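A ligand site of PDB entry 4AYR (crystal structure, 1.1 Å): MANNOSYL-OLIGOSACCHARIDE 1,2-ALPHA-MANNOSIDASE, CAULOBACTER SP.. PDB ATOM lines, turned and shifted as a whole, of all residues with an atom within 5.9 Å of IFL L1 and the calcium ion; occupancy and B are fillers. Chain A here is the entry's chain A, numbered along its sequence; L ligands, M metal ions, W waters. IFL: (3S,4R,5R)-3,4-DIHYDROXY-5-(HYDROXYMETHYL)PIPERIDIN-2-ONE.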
ATOM      1  N   PHE A  97      34.053 -14.830  39.087  1.00  0.00           N
ATOM      2  CA  PHE A  97      33.601 -15.374  37.810  1.00  0.00           C
ATOM      3  C   PHE A  97      33.998 -14.468  36.655  1.00  0.00           C
ATOM      4  O   PHE A  97      34.559 -14.919  35.633  1.00  0.00           O
ATOM      5  CB  PHE A  97      32.081 -15.537  37.884  1.00  0.00           C
ATOM      6  CG  PHE A  97      31.389 -15.733  36.559  1.00  0.00           C
ATOM      7  CD1 PHE A  97      31.302 -16.966  35.960  1.00  0.00           C
ATOM      8  CD2 PHE A  97      30.746 -14.665  35.965  1.00  0.00           C
ATOM      9  CE1 PHE A  97      30.627 -17.128  34.760  1.00  0.00           C
ATOM     10  CE2 PHE A  97      30.089 -14.813  34.758  1.00  0.00           C
ATOM     11  CZ  PHE A  97      30.024 -16.041  34.153  1.00  0.00           C
ATOM     12  N   GLU A  98      33.664 -13.181  36.755  1.00  0.00           N
ATOM     13  CA  GLU A  98      33.926 -12.259  35.659  1.00  0.00           C
ATOM     14  C   GLU A  98      35.425 -12.093  35.435  1.00  0.00           C
ATOM     15  O   GLU A  98      35.904 -11.998  34.303  1.00  0.00           O
ATOM     16  CB  GLU A  98      33.298 -10.878  35.918  1.00  0.00           C
ATOM     17  CG  GLU A  98      31.787 -10.839  36.068  1.00  0.00           C
ATOM     18  CD  GLU A  98      30.960 -11.117  34.842  1.00  0.00           C
ATOM     19  OE1 GLU A  98      31.504 -11.125  33.745  1.00  0.00           O
ATOM     20  OE2 GLU A  98      29.718 -11.278  35.003  1.00  0.00           O
ATOM     21  N   ILE A 101      36.706 -15.314  33.531  1.00  0.00           N
ATOM     22  CA  ILE A 101      36.349 -15.541  32.124  1.00  0.00           C
ATOM     23  C   ILE A 101      36.869 -14.415  31.236  1.00  0.00           C
ATOM     24  O   ILE A 101      37.170 -14.632  30.069  1.00  0.00           O
ATOM     25  CB  ILE A 101      34.852 -15.818  31.894  1.00  0.00           C
ATOM     26  CG1 ILE A 101      33.952 -14.609  32.166  1.00  0.00           C
ATOM     27  CG2 ILE A 101      34.421 -17.047  32.709  1.00  0.00           C
ATOM     28  CD1 ILE A 101      32.520 -14.810  31.779  1.00  0.00           C
ATOM     29  N   ARG A 102      36.972 -13.206  31.790  1.00  0.00           N
ATOM     30  CA  ARG A 102      37.391 -12.052  30.988  1.00  0.00           C
ATOM     31  C   ARG A 102      38.901 -11.838  30.990  1.00  0.00           C
ATOM     32  O   ARG A 102      39.517 -11.684  29.936  1.00  0.00           O
ATOM     33  CB  ARG A 102      36.710 -10.773  31.482  1.00  0.00           C
ATOM     34  CG  ARG A 102      35.188 -10.845  31.340  1.00  0.00           C
ATOM     35  CD  ARG A 102      34.507  -9.684  31.947  1.00  0.00           C
ATOM     36  NE  ARG A 102      33.060  -9.732  31.966  1.00  0.00           N
ATOM     37  CZ  ARG A 102      32.294  -9.008  31.178  1.00  0.00           C
ATOM     38  NH1 ARG A 102      32.780  -8.297  30.166  1.00  0.00           N
ATOM     39  NH2 ARG A 102      31.022  -8.994  31.440  1.00  0.00           N
ATOM     40  N   ASP A 226      24.030 -21.502  32.787  1.00  0.00           N
ATOM     41  CA  ASP A 226      24.558 -21.604  31.446  1.00  0.00           C
ATOM     42  C   ASP A 226      25.955 -22.228  31.281  1.00  0.00           C
ATOM     43  O   ASP A 226      26.076 -23.372  30.838  1.00  0.00           O
ATOM     44  CB  ASP A 226      24.411 -20.255  30.687  1.00  0.00           C
ATOM     45  CG  ASP A 226      24.917 -19.011  31.396  1.00  0.00           C
ATOM     46  OD1 ASP A 226      25.731 -19.062  32.339  1.00  0.00           O
ATOM     47  OD2 ASP A 226      24.489 -17.914  30.903  1.00  0.00           O
ATOM     48  N   SER A 227      27.003 -21.465  31.555  1.00  0.00           N
ATOM     49  CA  SER A 227      28.344 -21.894  31.193  1.00  0.00           C
ATOM     50  C   SER A 227      28.887 -23.070  32.000  1.00  0.00           C
ATOM     51  O   SER A 227      29.840 -23.708  31.544  1.00  0.00           O
ATOM     52  CB  SER A 227      29.293 -20.708  31.198  1.00  0.00           C
ATOM     53  OG  SER A 227      29.188 -19.953  32.404  1.00  0.00           O
ATOM     54  N   GLU A 230      28.416 -25.807  29.476  1.00  0.00           N
ATOM     55  CA  GLU A 230      29.466 -25.704  28.449  1.00  0.00           C
ATOM     56  C   GLU A 230      30.781 -26.269  28.940  1.00  0.00           C
ATOM     57  O   GLU A 230      31.449 -27.003  28.208  1.00  0.00           O
ATOM     58  CB  GLU A 230      29.727 -24.259  28.037  1.00  0.00           C
ATOM     59  CG  GLU A 230      28.629 -23.600  27.248  1.00  0.00           C
ATOM     60  CD  GLU A 230      29.034 -22.198  26.917  1.00  0.00           C
ATOM     61  OE1 GLU A 230      28.906 -21.337  27.839  1.00  0.00           O
ATOM     62  OE2 GLU A 230      29.540 -21.939  25.785  1.00  0.00           O
ATOM     63  N   GLU A 286      17.872 -13.987  26.238  1.00  0.00           N
ATOM     64  CA  GLU A 286      18.652 -14.090  25.010  1.00  0.00           C
ATOM     65  C   GLU A 286      19.920 -14.909  25.224  1.00  0.00           C
ATOM     66  O   GLU A 286      20.392 -15.566  24.304  1.00  0.00           O
ATOM     67  CB  GLU A 286      18.998 -12.688  24.509  1.00  0.00           C
ATOM     68  CG  GLU A 286      19.755 -12.644  23.189  1.00  0.00           C
ATOM     69  CD  GLU A 286      21.231 -12.984  23.316  1.00  0.00           C
ATOM     70  OE1 GLU A 286      21.759 -12.916  24.490  1.00  0.00           O
ATOM     71  OE2 GLU A 286      21.874 -13.318  22.304  1.00  0.00           O
ATOM     72  N   LEU A 287      20.462 -14.852  26.443  1.00  0.00           N
ATOM     73  CA  LEU A 287      21.723 -15.507  26.713  1.00  0.00           C
ATOM     74  C   LEU A 287      21.625 -17.022  26.603  1.00  0.00           C
ATOM     75  O   LEU A 287      22.644 -17.693  26.434  1.00  0.00           O
ATOM     76  CB  LEU A 287      22.292 -15.089  28.061  1.00  0.00           C
ATOM     77  CG  LEU A 287      22.813 -13.649  28.187  1.00  0.00           C
ATOM     78  CD1 LEU A 287      21.736 -12.571  28.118  1.00  0.00           C
ATOM     79  CD2 LEU A 287      23.593 -13.509  29.476  1.00  0.00           C
ATOM     80  N   TYR A 290      23.242 -19.678  23.601  1.00  0.00           N
ATOM     81  CA  TYR A 290      24.460 -20.484  23.576  1.00  0.00           C
ATOM     82  C   TYR A 290      24.120 -21.979  23.529  1.00  0.00           C
ATOM     83  O   TYR A 290      24.886 -22.784  22.981  1.00  0.00           O
ATOM     84  CB  TYR A 290      25.361 -20.224  24.831  1.00  0.00           C
ATOM     85  CG  TYR A 290      24.898 -21.046  26.035  1.00  0.00           C
ATOM     86  CD1 TYR A 290      23.780 -20.667  26.775  1.00  0.00           C
ATOM     87  CD2 TYR A 290      25.461 -22.275  26.325  1.00  0.00           C
ATOM     88  CE1 TYR A 290      23.240 -21.493  27.744  1.00  0.00           C
ATOM     89  CE2 TYR A 290      24.927 -23.120  27.297  1.00  0.00           C
ATOM     90  CZ  TYR A 290      23.806 -22.706  28.001  1.00  0.00           C
ATOM     91  OH  TYR A 290      23.264 -23.570  28.932  1.00  0.00           O
ATOM     92  N   GLY A 338      21.812  -5.836  26.017  1.00  0.00           N
ATOM     93  CA  GLY A 338      23.207  -5.798  26.358  1.00  0.00           C
ATOM     94  C   GLY A 338      24.144  -5.999  25.177  1.00  0.00           C
ATOM     95  O   GLY A 338      25.270  -6.437  25.384  1.00  0.00           O
ATOM     96  N   ARG A 340      24.281  -8.281  22.819  1.00  0.00           N
ATOM     97  CA  ARG A 340      24.610  -9.636  23.229  1.00  0.00           C
ATOM     98  C   ARG A 340      25.080 -10.517  22.081  1.00  0.00           C
ATOM     99  O   ARG A 340      24.562 -10.429  20.947  1.00  0.00           O
ATOM    100  CB  ARG A 340      23.417 -10.292  23.892  1.00  0.00           C
ATOM    101  CG  ARG A 340      22.993  -9.664  25.219  1.00  0.00           C
ATOM    102  CD  ARG A 340      23.953 -10.024  26.350  1.00  0.00           C
ATOM    103  NE  ARG A 340      23.531  -9.377  27.593  1.00  0.00           N
ATOM    104  CZ  ARG A 340      24.193  -9.457  28.740  1.00  0.00           C
ATOM    105  NH1 ARG A 340      25.294 -10.178  28.854  1.00  0.00           N
ATOM    106  NH2 ARG A 340      23.733  -8.796  29.797  1.00  0.00           N
ATOM    107  N   PRO A 341      26.024 -11.441  22.362  1.00  0.00           N
ATOM    108  CA  PRO A 341      26.672 -12.248  21.322  1.00  0.00           C
ATOM    109  C   PRO A 341      26.179 -13.676  21.150  1.00  0.00           C
ATOM    110  O   PRO A 341      26.757 -14.405  20.333  1.00  0.00           O
ATOM    111  CB  PRO A 341      28.120 -12.287  21.817  1.00  0.00           C
ATOM    112  CG  PRO A 341      27.947 -12.407  23.294  1.00  0.00           C
ATOM    113  CD  PRO A 341      26.824 -11.448  23.608  1.00  0.00           C
ATOM    114  N   GLU A 342      25.175 -14.134  21.901  1.00  0.00           N
ATOM    115  CA  GLU A 342      24.936 -15.585  21.967  1.00  0.00           C
ATOM    116  C   GLU A 342      24.362 -16.174  20.676  1.00  0.00           C
ATOM    117  O   GLU A 342      24.526 -17.377  20.455  1.00  0.00           O
ATOM    118  CB  GLU A 342      24.088 -15.955  23.161  1.00  0.00           C
ATOM    119  CG  GLU A 342      24.809 -15.824  24.489  1.00  0.00           C
ATOM    120  CD  GLU A 342      24.927 -14.412  25.047  1.00  0.00           C
ATOM    121  OE1 GLU A 342      24.272 -13.470  24.535  1.00  0.00           O
ATOM    122  OE2 GLU A 342      25.658 -14.257  26.044  1.00  0.00           O
ATOM    123  N   ASP A 345      27.316 -16.890  18.518  1.00  0.00           N
ATOM    124  CA  ASP A 345      27.993 -17.968  19.265  1.00  0.00           C
ATOM    125  C   ASP A 345      27.432 -19.313  18.801  1.00  0.00           C
ATOM    126  O   ASP A 345      28.153 -20.210  18.344  1.00  0.00           O
ATOM    127  CB  ASP A 345      27.737 -17.709  20.760  1.00  0.00           C
ATOM    128  CG  ASP A 345      28.231 -18.758  21.729  1.00  0.00           C
ATOM    129  OD1 ASP A 345      28.542 -19.890  21.320  1.00  0.00           O
ATOM    130  OD2 ASP A 345      28.249 -18.431  22.942  1.00  0.00           O
ATOM    131  N   TYR A 400      32.652  -7.799  26.640  1.00  0.00           N
ATOM    132  CA  TYR A 400      32.529  -9.062  25.902  1.00  0.00           C
ATOM    133  C   TYR A 400      32.364  -8.825  24.405  1.00  0.00           C
ATOM    134  O   TYR A 400      32.677  -9.731  23.624  1.00  0.00           O
ATOM    135  CB  TYR A 400      31.414  -9.977  26.452  1.00  0.00           C
ATOM    136  CG  TYR A 400      30.068  -9.319  26.677  1.00  0.00           C
ATOM    137  CD1 TYR A 400      29.219  -8.960  25.625  1.00  0.00           C
ATOM    138  CD2 TYR A 400      29.609  -9.092  27.971  1.00  0.00           C
ATOM    139  CE1 TYR A 400      27.966  -8.380  25.870  1.00  0.00           C
ATOM    140  CE2 TYR A 400      28.375  -8.506  28.220  1.00  0.00           C
ATOM    141  CZ  TYR A 400      27.566  -8.137  27.166  1.00  0.00           C
ATOM    142  OH  TYR A 400      26.363  -7.546  27.463  1.00  0.00           O
ATOM    143  N   GLU A 404      33.819 -11.493  21.727  1.00  0.00           N
ATOM    144  CA  GLU A 404      32.805 -12.437  21.241  1.00  0.00           C
ATOM    145  C   GLU A 404      32.298 -12.149  19.833  1.00  0.00           C
ATOM    146  O   GLU A 404      32.749 -12.784  18.885  1.00  0.00           O
ATOM    147  CB  GLU A 404      31.675 -12.575  22.242  1.00  0.00           C
ATOM    148  CG  GLU A 404      32.141 -13.145  23.584  1.00  0.00           C
ATOM    149  CD  GLU A 404      31.048 -13.886  24.340  1.00  0.00           C
ATOM    150  OE1 GLU A 404      30.338 -14.710  23.709  1.00  0.00           O
ATOM    151  OE2 GLU A 404      30.914 -13.619  25.553  1.00  0.00           O
ATOM    152  N   TYR A 408      33.217 -14.053  16.378  1.00  0.00           N
ATOM    153  CA  TYR A 408      32.343 -15.079  15.798  1.00  0.00           C
ATOM    154  C   TYR A 408      32.068 -14.781  14.332  1.00  0.00           C
ATOM    155  O   TYR A 408      32.158 -15.672  13.486  1.00  0.00           O
ATOM    156  CB  TYR A 408      31.018 -15.202  16.545  1.00  0.00           C
ATOM    157  CG  TYR A 408      31.098 -15.561  18.012  1.00  0.00           C
ATOM    158  CD1 TYR A 408      32.021 -16.458  18.502  1.00  0.00           C
ATOM    159  CD2 TYR A 408      30.167 -15.027  18.906  1.00  0.00           C
ATOM    160  CE1 TYR A 408      32.064 -16.791  19.854  1.00  0.00           C
ATOM    161  CE2 TYR A 408      30.186 -15.347  20.252  1.00  0.00           C
ATOM    162  CZ  TYR A 408      31.140 -16.227  20.727  1.00  0.00           C
ATOM    163  OH  TYR A 408      31.211 -16.544  22.074  1.00  0.00           O
ATOM    164  N   SER A 427      36.438 -20.442  24.792  1.00  0.00           N
ATOM    165  CA  SER A 427      35.870 -20.350  26.135  1.00  0.00           C
ATOM    166  C   SER A 427      34.455 -19.738  26.048  1.00  0.00           C
ATOM    167  O   SER A 427      33.993 -19.343  24.982  1.00  0.00           O
ATOM    168  CB  SER A 427      36.757 -19.491  27.032  1.00  0.00           C
ATOM    169  OG  SER A 427      36.473 -18.104  26.815  1.00  0.00           O
ATOM    170  N   THR A 428      33.782 -19.611  27.187  1.00  0.00           N
ATOM    171  CA  THR A 428      32.443 -19.020  27.172  1.00  0.00           C
ATOM    172  C   THR A 428      32.478 -17.516  26.845  1.00  0.00           C
ATOM    173  O   THR A 428      31.432 -16.932  26.561  1.00  0.00           O
ATOM    174  CB  THR A 428      31.658 -19.283  28.474  1.00  0.00           C
ATOM    175  OG1 THR A 428      30.269 -19.076  28.225  1.00  0.00           O
ATOM    176  CG2 THR A 428      32.101 -18.387  29.613  1.00  0.00           C
ATOM    177  N   GLU A 429      33.668 -16.914  26.921  1.00  0.00           N
ATOM    178  CA  GLU A 429      33.930 -15.520  26.576  1.00  0.00           C
ATOM    179  C   GLU A 429      34.583 -15.430  25.186  1.00  0.00           C
ATOM    180  O   GLU A 429      35.094 -14.377  24.788  1.00  0.00           O
ATOM    181  CB  GLU A 429      34.857 -14.917  27.641  1.00  0.00           C
ATOM    182  CG  GLU A 429      34.996 -13.397  27.647  1.00  0.00           C
ATOM    183  CD  GLU A 429      33.811 -12.657  28.203  1.00  0.00           C
ATOM    184  OE1 GLU A 429      32.902 -13.274  28.775  1.00  0.00           O
ATOM    185  OE2 GLU A 429      33.800 -11.389  28.115  1.00  0.00           O
HETATM  186  O4  IFL L   1      30.478 -12.430  29.716  1.00  0.00           O
HETATM  187  C4  IFL L   1      29.853 -12.904  28.506  1.00  0.00           C
HETATM  188  C3  IFL L   1      29.957 -14.439  28.476  1.00  0.00           C
HETATM  189  O3  IFL L   1      29.490 -14.943  27.213  1.00  0.00           O
HETATM  190  C2  IFL L   1      29.114 -15.128  29.484  1.00  0.00           C
HETATM  191  N   IFL L   1      27.727 -14.671  29.429  1.00  0.00           N
HETATM  192  C7  IFL L   1      27.495 -13.202  29.454  1.00  0.00           C
HETATM  193  C5  IFL L   1      28.400 -12.428  28.485  1.00  0.00           C
HETATM  194  C6  IFL L   1      27.872 -12.378  27.053  1.00  0.00           C
HETATM  195  O6  IFL L   1      26.502 -11.947  27.004  1.00  0.00           O
HETATM  196  O2  IFL L   1      29.193 -16.489  29.329  1.00  0.00           O
HETATM  197  O4  IFL L   2      25.194 -17.034  34.130  1.00  0.00           O
HETATM  198  C4  IFL L   2      25.961 -15.844  33.987  1.00  0.00           C
HETATM  199  C3  IFL L   2      25.598 -15.106  32.685  1.00  0.00           C
HETATM  200  O3  IFL L   2      25.968 -15.799  31.496  1.00  0.00           O
HETATM  201  C2  IFL L   2      26.329 -13.820  32.680  1.00  0.00           C
HETATM  202  N   IFL L   2      25.942 -12.965  33.727  1.00  0.00           N
HETATM  203  C7  IFL L   2      26.351 -13.535  35.034  1.00  0.00           C
HETATM  204  C5  IFL L   2      25.717 -14.898  35.183  1.00  0.00           C
HETATM  205  C6  IFL L   2      26.177 -15.584  36.462  1.00  0.00           C
HETATM  206  O6  IFL L   2      25.806 -14.840  37.636  1.00  0.00           O
HETATM  207  O2  IFL L   2      27.689 -14.032  32.479  1.00  0.00           O
HETATM  208 CA    CA M   1      29.037 -17.347  26.944  1.00  0.00          CA
HETATM  209  O   HOH W   1      28.523 -16.382  24.791  1.00  0.00           O
HETATM  210  O   HOH W   2      26.833 -16.245  27.295  1.00  0.00           O
HETATM  211  O   HOH W   3      29.138 -11.835  32.097  1.00  0.00           O
HETATM  212  O   HOH W   4      27.430 -18.991  27.857  1.00  0.00           O
HETATM  213  O   HOH W   5      29.276 -19.159  25.362  1.00  0.00           O
HETATM  214  O   HOH W   6      28.412 -17.502  31.589  1.00  0.00           O
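Water W5 bridges the side-chain carboxylate of Asp 345 and the side-chain carboxylate of Glu 230. Water W1 lies within hydrogen-bond range of OE1 of Glu 404 (2.7 Å) and OD2 of Asp 345 (2.8 Å). Water W2 bridges OE2 of Glu 342 (2.6 Å) and N of IFL L1 (2.8 Å). Water W6 lies within hydrogen-bond range of OG of Ser 227 (2.7 Å), O3 of IFL L2 (3.0 Å) and OD1 of Asp 226 (3.2 Å). Water W3 lies within hydrogen-bond range of O2 of IFL L2, O4 of IFL L1, OE1 of Glu 98 and NH2 of Arg 102.
The calcium ion is bound by water W1 (2.4 Å). The calcium ion is bound by water W5, 2.4 Å away. The backbone carbonyl oxygen (O) of Thr 428 binds the calcium ion. The calcium ion is bound by an oxygen (O3) of IFL L1. The calcium ion is bound by water W4, at 2.5 Å. OG1 of Thr 428 is bound to the calcium ion, 2.5 Å away. Water W2 binds the calcium ion (2.5 Å). The calcium ion is bound by O2 of IFL L1 (2.5 Å). The calcium ion has eight donor atoms within binding distance.
An oxygen (O3) of IFL L2 is in hydrogen-bond range of a nitrogen (N) of IFL L1 (2.9 Å).
The side-chain carboxylate (OE2) of Glu 404 lies close to an oxygen (O3) of IFL L1, 2.6 Å away. The side-chain carboxylate of Glu 342 lies within hydrogen-bond range of an oxygen (O6) of IFL L1. The side-chain carboxylate (OE1) of Glu 429 sits at hydrogen-bond distance from an oxygen (O4) of IFL L1 (2.7 Å). The guanidinium group (NH1) of Arg 340 lies within hydrogen-bond range of an oxygen (O6) of IFL L1. The side-chain carboxylate (OD2) of Asp 226 sits at hydrogen-bond distance from an oxygen (O3) of IFL L2 (2.6 Å).
OG1 of Thr 428 lies close to OE1 of Glu 230 (2.7 Å). The side-chain hydroxyl of Tyr 408 is in hydrogen-bond range of the side-chain carboxylate of Glu 404. OE2 of Glu 286 sits at hydrogen-bond distance from N of Glu 342. The side-chain carboxylate of Glu 429 is in salt-bridge range of the guanidinium group of Arg 102 (3.8 Å). The side-chain hydroxyl (OG) of Ser 427 lies within hydrogen-bond range of the backbone NH (N) of Glu 429 (3.0 Å). NH1 of Arg 340 sits close to OH of Tyr 400, 3.2 Å away. The backbone carbonyl oxygen (O) of Gly 338 sits at hydrogen-bond distance from the side-chain hydroxyl (OH) of Tyr 400 (2.6 Å). OE1 of Glu 98 is in salt-bridge range of NE of Arg 102 (2.7 Å).
Merely in contact with IFL L1: Pro 341 (3.4 Å), Tyr 400 (3.6 Å), Ile 101 (3.8 Å), Arg 102 (3.9 Å) and Leu 287 (3.9 Å). Hydrophobic or aromatic side chains within 4 Å of IFL L1: Ile 101, Leu 287, Pro 341 and Tyr 400. Ten residues have an atom within 4 Å of IFL L1: Ile 101, Arg 102, Leu 287, Arg 340, Pro 341, Glu 342, Tyr 400, Glu 404, Thr 428 and Glu 429.
Within 4 Å of the calcium ion: Thr 428.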
